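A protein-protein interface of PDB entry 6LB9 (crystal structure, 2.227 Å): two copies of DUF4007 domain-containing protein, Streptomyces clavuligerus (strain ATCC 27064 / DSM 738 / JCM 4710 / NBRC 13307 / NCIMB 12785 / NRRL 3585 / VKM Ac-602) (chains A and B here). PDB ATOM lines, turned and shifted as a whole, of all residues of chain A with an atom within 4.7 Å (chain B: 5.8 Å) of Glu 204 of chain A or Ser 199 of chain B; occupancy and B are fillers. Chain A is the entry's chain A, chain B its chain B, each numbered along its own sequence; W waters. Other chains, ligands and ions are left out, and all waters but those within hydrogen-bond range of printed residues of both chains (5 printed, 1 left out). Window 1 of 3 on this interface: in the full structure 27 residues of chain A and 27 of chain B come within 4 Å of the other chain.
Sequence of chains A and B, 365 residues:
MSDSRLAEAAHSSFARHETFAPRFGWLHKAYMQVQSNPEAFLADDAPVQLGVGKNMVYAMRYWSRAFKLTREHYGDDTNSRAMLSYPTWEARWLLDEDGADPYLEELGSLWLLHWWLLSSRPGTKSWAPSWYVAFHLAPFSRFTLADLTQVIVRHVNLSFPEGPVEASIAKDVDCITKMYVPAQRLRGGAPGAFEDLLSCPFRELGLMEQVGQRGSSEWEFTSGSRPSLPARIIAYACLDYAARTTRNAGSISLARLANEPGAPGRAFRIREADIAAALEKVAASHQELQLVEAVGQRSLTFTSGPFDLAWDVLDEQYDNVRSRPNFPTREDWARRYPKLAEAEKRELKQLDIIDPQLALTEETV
Of the printed residues of chain B, Leu 107 of chain A touches Ala 183, Leu 197, Leu 198 and Ser 199.
Of the printed residues of chain B, Arg 203 of chain A touches Glu 204 (2.7 Å).
Of the printed residues of chain A, Gln 184 of chain B touches Glu 204, Leu 205 and Gly 206.
Printed residues of chain A within 4 Å of Leu 198 of chain B: Glu 105 (3.4 Å), Glu 106 (3.8 Å) and Leu 107 (3.7 Å).
Ser 199 of chain B touches just these residues of chain A: Leu 104 (3.9 Å), Glu 105 (2.9 Å), Leu 107 (3.8 Å) and Glu 204 (2.8 Å).
The nearest residue of chain B that does not touch Glu 204 of chain A is Ala 183 of chain B (4.3 Å).
The nearest printed residue of chain B that does not touch Leu 205 of chain A is Ala 183 of chain B (6.9 Å).
The side-chain carboxylate of Glu 105 of chain A is in salt-bridge range of the guanidinium group of Arg 23 of chain B.
The backbone NH (N) of Ser 199 of chain B is in hydrogen-bond range of the backbone carbonyl oxygen (O) of Glu 105 of chain A (2.9 Å).
The backbone NH of Leu 107 of chain A is in hydrogen-bond range of the backbone carbonyl oxygen of Leu 197 of chain B (3.1 Å).
N of Cys 200 of chain A lies within hydrogen-bond range of OE1 of Glu 204 of chain B (2.7 Å).
The guanidinium group of Arg 203 of chain A is in salt-bridge range of the side-chain carboxylate of Glu 204 of chain B, at 2.7 Å.
The backbone carbonyl oxygen (O) of Glu 204 of chain A lies close to the side-chain amide oxygen (OE1) of Gln 184 of chain B, at 2.9 Å.
The side-chain carboxylate (OE1) of Glu 204 of chain A is in hydrogen-bond range of the side-chain hydroxyl (OG) of Ser 199 of chain B (2.8 Å).
The side-chain carboxylate (OE1) of Glu 204 of chain A sits at hydrogen-bond distance from the backbone NH (N) of Cys 200 of chain B.
OE2 of Glu 204 of chain A lies within salt-bridge range of NH1 of Arg 203 of chain B.
Of the 11 printed residues of chain B, 9 touch a printed residue of chain A.
Of the 11 printed residues of chain A, 9 touch a printed residue of chain B.
Hydrophobic or aromatic side chains of chain A within 4 Å of the printed part of chain B: Leu 107.
Among the printed residues, 18 pairs touch across the chains.
Water W4 bridges the backbone carbonyl oxygen of Ser 199 of chain B and the backbone carbonyl oxygen of Glu 105 of chain A.
Water W2 lies within hydrogen-bond range of the backbone NH (N) of Ala 183 of chain B (2.6 Å) and the side-chain carboxylate (OE2) of Glu 204 of chain A (3.0 Å).
Water W5 bridges O of Leu 197 of chain B (2.6 Å) and N of Leu 107 of chain A (3.3 Å).
Water W3 lies within hydrogen-bond range of the backbone carbonyl oxygen of Leu 104 of chain A (2.7 Å) and the side-chain hydroxyl of Ser 199 of chain B (3.2 Å).
Water W1 lies within hydrogen-bond range of OE1 of Glu 204 of chain A (3.0 Å) and OG of Ser 199 of chain B (3.3 Å).
Cys 200 of chain A touches Glu 204 of chain B, and with the chains exchanged Glu 204 of chain A touches Cys 200 of chain B.
Arg 203 of chain A touches Glu 204 of chain B, and with the chains exchanged Glu 204 of chain A touches Arg 203 of chain B.
Among the printed residues, pairs that only touch across the chains: Leu 104 of chain A with Ser 199 of chain B (3.9 Å), Glu 105 of chain A with Leu 198 of chain B (3.4 Å), Glu 106 of chain A with Leu 197 of chain B (3.9 Å), Glu 106 of chain A with Leu 198 of chain B (3.8 Å), Leu 107 of chain A with Ala 183 of chain B (3.7 Å), Leu 107 of chain A with Leu 198 of chain B (3.7 Å), Leu 107 of chain A with Ser 199 of chain B (3.8 Å), Leu 205 of chain A with Gln 184 of chain B (3.6 Å) and Gly 206 of chain A with Gln 184 of chain B (3.9 Å).
The side-chain sulfur (SG) of Cys 200 of chain B is in hydrogen-bond range of the backbone carbonyl oxygen (O) of Pro 22 of chain B (3.5 Å).
The backbone carbonyl oxygen of Leu 198 of chain B is in hydrogen-bond range of the guanidinium group of Arg 203 of chain B, at 2.8 Å.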
ATOM      1  N   LEU A 104     -19.961  -5.714  -5.100  1.00  0.00           N
ATOM      2  CA  LEU A 104     -21.377  -5.523  -4.754  1.00  0.00           C
ATOM      3  C   LEU A 104     -21.752  -4.043  -4.753  1.00  0.00           C
ATOM      4  O   LEU A 104     -22.286  -3.510  -3.781  1.00  0.00           O
ATOM      5  CB  LEU A 104     -21.705  -6.171  -3.413  1.00  0.00           C
ATOM      6  CG  LEU A 104     -21.338  -7.656  -3.323  1.00  0.00           C
ATOM      7  CD1 LEU A 104     -21.890  -8.270  -2.042  1.00  0.00           C
ATOM      8  CD2 LEU A 104     -21.812  -8.425  -4.581  1.00  0.00           C
ATOM      9  N   GLU A 105     -21.415  -3.371  -5.851  1.00  0.00           N
ATOM     10  CA  GLU A 105     -21.673  -1.941  -5.970  1.00  0.00           C
ATOM     11  C   GLU A 105     -23.137  -1.632  -6.255  1.00  0.00           C
ATOM     12  O   GLU A 105     -23.609  -0.537  -5.922  1.00  0.00           O
ATOM     13  CB  GLU A 105     -20.802  -1.348  -7.080  1.00  0.00           C
ATOM     14  CG  GLU A 105     -19.334  -1.327  -6.724  1.00  0.00           C
ATOM     15  CD  GLU A 105     -18.462  -0.689  -7.803  1.00  0.00           C
ATOM     16  OE1 GLU A 105     -19.002  -0.056  -8.750  1.00  0.00           O
ATOM     17  OE2 GLU A 105     -17.229  -0.830  -7.680  1.00  0.00           O
ATOM     18  N   GLU A 106     -23.861  -2.554  -6.883  1.00  0.00           N
ATOM     19  CA  GLU A 106     -25.249  -2.309  -7.246  1.00  0.00           C
ATOM     20  C   GLU A 106     -26.159  -3.065  -6.290  1.00  0.00           C
ATOM     21  O   GLU A 106     -25.883  -4.211  -5.931  1.00  0.00           O
ATOM     22  CB  GLU A 106     -25.529  -2.728  -8.693  1.00  0.00           C
ATOM     23  CG  GLU A 106     -24.820  -1.882  -9.746  1.00  0.00           C
ATOM     24  CD  GLU A 106     -25.121  -2.340 -11.171  1.00  0.00           C
ATOM     25  OE1 GLU A 106     -26.085  -3.132 -11.356  1.00  0.00           O
ATOM     26  OE2 GLU A 106     -24.411  -1.888 -12.106  1.00  0.00           O
ATOM     27  N   LEU A 107     -27.241  -2.417  -5.868  1.00  0.00           N
ATOM     28  CA  LEU A 107     -28.124  -3.073  -4.911  1.00  0.00           C
ATOM     29  C   LEU A 107     -28.824  -4.292  -5.507  1.00  0.00           C
ATOM     30  O   LEU A 107     -29.211  -5.191  -4.754  1.00  0.00           O
ATOM     31  CB  LEU A 107     -29.137  -2.067  -4.364  1.00  0.00           C
ATOM     32  CG  LEU A 107     -28.532  -1.032  -3.401  1.00  0.00           C
ATOM     33  CD1 LEU A 107     -29.526   0.072  -3.087  1.00  0.00           C
ATOM     34  CD2 LEU A 107     -28.054  -1.716  -2.116  1.00  0.00           C
ATOM     35  N   CYS A 200     -23.393  -4.737   7.345  1.00  0.00           N
ATOM     36  CA  CYS A 200     -23.954  -5.861   6.616  1.00  0.00           C
ATOM     37  C   CYS A 200     -24.708  -5.234   5.456  1.00  0.00           C
ATOM     38  O   CYS A 200     -25.722  -4.548   5.674  1.00  0.00           O
ATOM     39  CB  CYS A 200     -24.872  -6.734   7.486  1.00  0.00           C
ATOM     40  SG  CYS A 200     -25.575  -8.190   6.582  1.00  0.00           S
ATOM     41  N   PRO A 201     -24.258  -5.446   4.219  1.00  0.00           N
ATOM     42  CA  PRO A 201     -24.868  -4.722   3.102  1.00  0.00           C
ATOM     43  C   PRO A 201     -26.298  -5.146   2.800  1.00  0.00           C
ATOM     44  O   PRO A 201     -26.991  -4.411   2.093  1.00  0.00           O
ATOM     45  CB  PRO A 201     -23.922  -5.012   1.925  1.00  0.00           C
ATOM     46  CG  PRO A 201     -23.227  -6.268   2.287  1.00  0.00           C
ATOM     47  CD  PRO A 201     -23.103  -6.258   3.800  1.00  0.00           C
ATOM     48  N   PHE A 202     -26.782  -6.282   3.320  1.00  0.00           N
ATOM     49  CA  PHE A 202     -28.183  -6.655   3.094  1.00  0.00           C
ATOM     50  C   PHE A 202     -29.169  -5.741   3.817  1.00  0.00           C
ATOM     51  O   PHE A 202     -30.367  -5.789   3.519  1.00  0.00           O
ATOM     52  CB  PHE A 202     -28.406  -8.127   3.503  1.00  0.00           C
ATOM     53  CG  PHE A 202     -27.715  -9.095   2.579  1.00  0.00           C
ATOM     54  CD1 PHE A 202     -28.319  -9.480   1.379  1.00  0.00           C
ATOM     55  CD2 PHE A 202     -26.441  -9.541   2.856  1.00  0.00           C
ATOM     56  CE1 PHE A 202     -27.685 -10.346   0.509  1.00  0.00           C
ATOM     57  CE2 PHE A 202     -25.784 -10.405   1.988  1.00  0.00           C
ATOM     58  CZ  PHE A 202     -26.400 -10.806   0.821  1.00  0.00           C
ATOM     59  N   ARG A 203     -28.693  -4.929   4.763  1.00  0.00           N
ATOM     60  CA  ARG A 203     -29.545  -3.981   5.471  1.00  0.00           C
ATOM     61  C   ARG A 203     -30.083  -2.907   4.542  1.00  0.00           C
ATOM     62  O   ARG A 203     -31.147  -2.328   4.809  1.00  0.00           O
ATOM     63  CB  ARG A 203     -28.756  -3.338   6.609  1.00  0.00           C
ATOM     64  CG  ARG A 203     -28.335  -4.331   7.682  1.00  0.00           C
ATOM     65  CD  ARG A 203     -27.551  -3.643   8.775  1.00  0.00           C
ATOM     66  NE  ARG A 203     -27.134  -4.622   9.763  1.00  0.00           N
ATOM     67  CZ  ARG A 203     -25.988  -4.582  10.432  1.00  0.00           C
ATOM     68  NH1 ARG A 203     -25.126  -3.593  10.228  1.00  0.00           N
ATOM     69  NH2 ARG A 203     -25.705  -5.541  11.302  1.00  0.00           N
ATOM     70  N   GLU A 204     -29.354  -2.631   3.457  1.00  0.00           N
ATOM     71  CA  GLU A 204     -29.769  -1.685   2.422  1.00  0.00           C
ATOM     72  C   GLU A 204     -31.047  -2.097   1.692  1.00  0.00           C
ATOM     73  O   GLU A 204     -31.680  -1.251   1.047  1.00  0.00           O
ATOM     74  CB  GLU A 204     -28.644  -1.541   1.401  1.00  0.00           C
ATOM     75  CG  GLU A 204     -27.470  -0.773   1.931  1.00  0.00           C
ATOM     76  CD  GLU A 204     -26.981   0.290   0.961  1.00  0.00           C
ATOM     77  OE1 GLU A 204     -25.769   0.306   0.653  1.00  0.00           O
ATOM     78  OE2 GLU A 204     -27.808   1.120   0.517  1.00  0.00           O
ATOM     79  N   LEU A 205     -31.428  -3.376   1.747  1.00  0.00           N
ATOM     80  CA  LEU A 205     -32.623  -3.814   1.037  1.00  0.00           C
ATOM     81  C   LEU A 205     -33.915  -3.382   1.731  1.00  0.00           C
ATOM     82  O   LEU A 205     -34.987  -3.551   1.147  1.00  0.00           O
ATOM     83  CB  LEU A 205     -32.609  -5.343   0.871  1.00  0.00           C
ATOM     84  CG  LEU A 205     -31.397  -6.008   0.197  1.00  0.00           C
ATOM     85  CD1 LEU A 205     -31.630  -7.502   0.064  1.00  0.00           C
ATOM     86  CD2 LEU A 205     -31.126  -5.376  -1.173  1.00  0.00           C
ATOM     87  N   GLY A 206     -33.843  -2.872   2.961  1.00  0.00           N
ATOM     88  CA  GLY A 206     -35.019  -2.351   3.655  1.00  0.00           C
ATOM     89  C   GLY A 206     -36.080  -3.387   3.938  1.00  0.00           C
ATOM     90  O   GLY A 206     -37.269  -3.057   3.996  1.00  0.00           O
ATOM     91  N   PRO B  22     -19.751   7.901  -2.559  1.00  0.00           N
ATOM     92  CA  PRO B  22     -18.619   6.968  -2.446  1.00  0.00           C
ATOM     93  C   PRO B  22     -19.078   5.524  -2.611  1.00  0.00           C
ATOM     94  O   PRO B  22     -20.230   5.187  -2.327  1.00  0.00           O
ATOM     95  CB  PRO B  22     -18.072   7.228  -1.034  1.00  0.00           C
ATOM     96  CG  PRO B  22     -18.743   8.471  -0.538  1.00  0.00           C
ATOM     97  CD  PRO B  22     -20.070   8.515  -1.260  1.00  0.00           C
ATOM     98  N   ARG B  23     -18.171   4.682  -3.128  1.00  0.00           N
ATOM     99  CA  ARG B  23     -18.369   3.238  -3.278  1.00  0.00           C
ATOM    100  C   ARG B  23     -17.185   2.506  -2.650  1.00  0.00           C
ATOM    101  O   ARG B  23     -16.039   2.941  -2.805  1.00  0.00           O
ATOM    102  CB  ARG B  23     -18.476   2.824  -4.760  1.00  0.00           C
ATOM    103  CG  ARG B  23     -19.472   3.632  -5.603  1.00  0.00           C
ATOM    104  CD  ARG B  23     -19.707   2.972  -6.958  1.00  0.00           C
ATOM    105  NE  ARG B  23     -20.302   3.915  -7.901  1.00  0.00           N
ATOM    106  CZ  ARG B  23     -20.625   3.641  -9.159  1.00  0.00           C
ATOM    107  NH1 ARG B  23     -20.399   2.430  -9.679  1.00  0.00           N
ATOM    108  NH2 ARG B  23     -21.170   4.596  -9.903  1.00  0.00           N
ATOM    109  N   ALA B 183     -31.749   4.022   0.705  1.00  0.00           N
ATOM    110  CA  ALA B 183     -32.039   3.945  -0.722  1.00  0.00           C
ATOM    111  C   ALA B 183     -33.526   3.831  -1.014  1.00  0.00           C
ATOM    112  O   ALA B 183     -33.953   4.137  -2.128  1.00  0.00           O
ATOM    113  CB  ALA B 183     -31.301   2.757  -1.342  1.00  0.00           C
ATOM    114  N   GLN B 184     -34.326   3.380  -0.054  1.00  0.00           N
ATOM    115  CA  GLN B 184     -35.769   3.372  -0.266  1.00  0.00           C
ATOM    116  C   GLN B 184     -36.331   4.777  -0.428  1.00  0.00           C
ATOM    117  O   GLN B 184     -37.439   4.925  -0.958  1.00  0.00           O
ATOM    118  CB  GLN B 184     -36.479   2.649   0.886  1.00  0.00           C
ATOM    119  CG  GLN B 184     -36.238   1.146   0.874  1.00  0.00           C
ATOM    120  CD  GLN B 184     -34.768   0.784   1.091  1.00  0.00           C
ATOM    121  OE1 GLN B 184     -34.203  -0.039   0.357  1.00  0.00           O
ATOM    122  NE2 GLN B 184     -34.156   1.374   2.108  1.00  0.00           N
ATOM    123  N   LEU B 197     -29.834   1.876  -9.017  1.00  0.00           N
ATOM    124  CA  LEU B 197     -29.489   2.231  -7.635  1.00  0.00           C
ATOM    125  C   LEU B 197     -28.260   1.491  -7.120  1.00  0.00           C
ATOM    126  O   LEU B 197     -28.195   0.255  -7.133  1.00  0.00           O
ATOM    127  CB  LEU B 197     -30.671   2.019  -6.685  1.00  0.00           C
ATOM    128  CG  LEU B 197     -31.752   3.107  -6.636  1.00  0.00           C
ATOM    129  CD1 LEU B 197     -32.638   3.013  -5.356  1.00  0.00           C
ATOM    130  CD2 LEU B 197     -31.122   4.481  -6.754  1.00  0.00           C
ATOM    131  N   LEU B 198     -27.290   2.280  -6.656  1.00  0.00           N
ATOM    132  CA  LEU B 198     -26.023   1.827  -6.102  1.00  0.00           C
ATOM    133  C   LEU B 198     -26.090   1.735  -4.588  1.00  0.00           C
ATOM    134  O   LEU B 198     -26.833   2.468  -3.933  1.00  0.00           O
ATOM    135  CB  LEU B 198     -24.873   2.771  -6.494  1.00  0.00           C
ATOM    136  CG  LEU B 198     -24.780   3.028  -7.998  1.00  0.00           C
ATOM    137  CD1 LEU B 198     -23.894   4.225  -8.261  1.00  0.00           C
ATOM    138  CD2 LEU B 198     -24.300   1.778  -8.721  1.00  0.00           C
ATOM    139  N   SER B 199     -25.299   0.815  -4.047  1.00  0.00           N
ATOM    140  CA  SER B 199     -25.024   0.739  -2.621  1.00  0.00           C
ATOM    141  C   SER B 199     -24.144   1.910  -2.171  1.00  0.00           C
ATOM    142  O   SER B 199     -23.340   2.454  -2.941  1.00  0.00           O
ATOM    143  CB  SER B 199     -24.325  -0.590  -2.311  1.00  0.00           C
ATOM    144  OG  SER B 199     -23.729  -0.559  -1.034  1.00  0.00           O
ATOM    145  N   CYS B 200     -24.313   2.322  -0.912  1.00  0.00           N
ATOM    146  CA  CYS B 200     -23.360   3.286  -0.358  1.00  0.00           C
ATOM    147  C   CYS B 200     -23.222   3.014   1.123  1.00  0.00           C
ATOM    148  O   CYS B 200     -24.183   3.199   1.870  1.00  0.00           O
ATOM    149  CB  CYS B 200     -23.774   4.744  -0.556  1.00  0.00           C
ATOM    150  SG  CYS B 200     -22.551   5.918   0.177  1.00  0.00           S
ATOM    151  N   PRO B 201     -22.049   2.597   1.589  1.00  0.00           N
ATOM    152  CA  PRO B 201     -21.961   2.078   2.960  1.00  0.00           C
ATOM    153  C   PRO B 201     -22.179   3.121   4.031  1.00  0.00           C
ATOM    154  O   PRO B 201     -22.420   2.746   5.180  1.00  0.00           O
ATOM    155  CB  PRO B 201     -20.534   1.507   3.036  1.00  0.00           C
ATOM    156  CG  PRO B 201     -19.790   2.278   2.037  1.00  0.00           C
ATOM    157  CD  PRO B 201     -20.756   2.533   0.895  1.00  0.00           C
ATOM    158  N   ARG B 203     -24.705   4.927   4.346  1.00  0.00           N
ATOM    159  CA  ARG B 203     -26.112   4.949   4.748  1.00  0.00           C
ATOM    160  C   ARG B 203     -26.331   4.183   6.042  1.00  0.00           C
ATOM    161  O   ARG B 203     -27.314   4.443   6.745  1.00  0.00           O
ATOM    162  CB  ARG B 203     -27.011   4.366   3.652  1.00  0.00           C
ATOM    163  CG  ARG B 203     -26.983   5.166   2.354  1.00  0.00           C
ATOM    164  CD  ARG B 203     -27.663   4.432   1.195  1.00  0.00           C
ATOM    165  NE  ARG B 203     -27.473   5.165  -0.062  1.00  0.00           N
ATOM    166  CZ  ARG B 203     -27.496   4.619  -1.277  1.00  0.00           C
ATOM    167  NH1 ARG B 203     -27.705   3.320  -1.428  1.00  0.00           N
ATOM    168  NH2 ARG B 203     -27.312   5.383  -2.346  1.00  0.00           N
ATOM    169  N   GLU B 204     -25.421   3.262   6.381  1.00  0.00           N
ATOM    170  CA  GLU B 204     -25.565   2.456   7.589  1.00  0.00           C
ATOM    171  C   GLU B 204     -25.366   3.275   8.851  1.00  0.00           C
ATOM    172  O   GLU B 204     -25.713   2.803   9.944  1.00  0.00           O
ATOM    173  CB  GLU B 204     -24.568   1.284   7.579  1.00  0.00           C
ATOM    174  CG  GLU B 204     -25.025   0.056   6.767  1.00  0.00           C
ATOM    175  CD  GLU B 204     -24.652  -1.273   7.453  1.00  0.00           C
ATOM    176  OE1 GLU B 204     -24.083  -2.162   6.799  1.00  0.00           O
ATOM    177  OE2 GLU B 204     -24.930  -1.428   8.662  1.00  0.00           O
HETATM  178  O   HOH W   1     -23.356  -0.623   2.222  1.00  0.00           O
HETATM  179  O   HOH W   2     -30.440   2.008   1.718  1.00  0.00           O
HETATM  180  O   HOH W   3     -22.602  -3.544  -1.053  1.00  0.00           O
HETATM  181  O   HOH W   4     -21.951   1.144  -4.646  1.00  0.00           O
HETATM  182  O   HOH W   5     -29.239  -1.779  -8.421  1.00  0.00           O
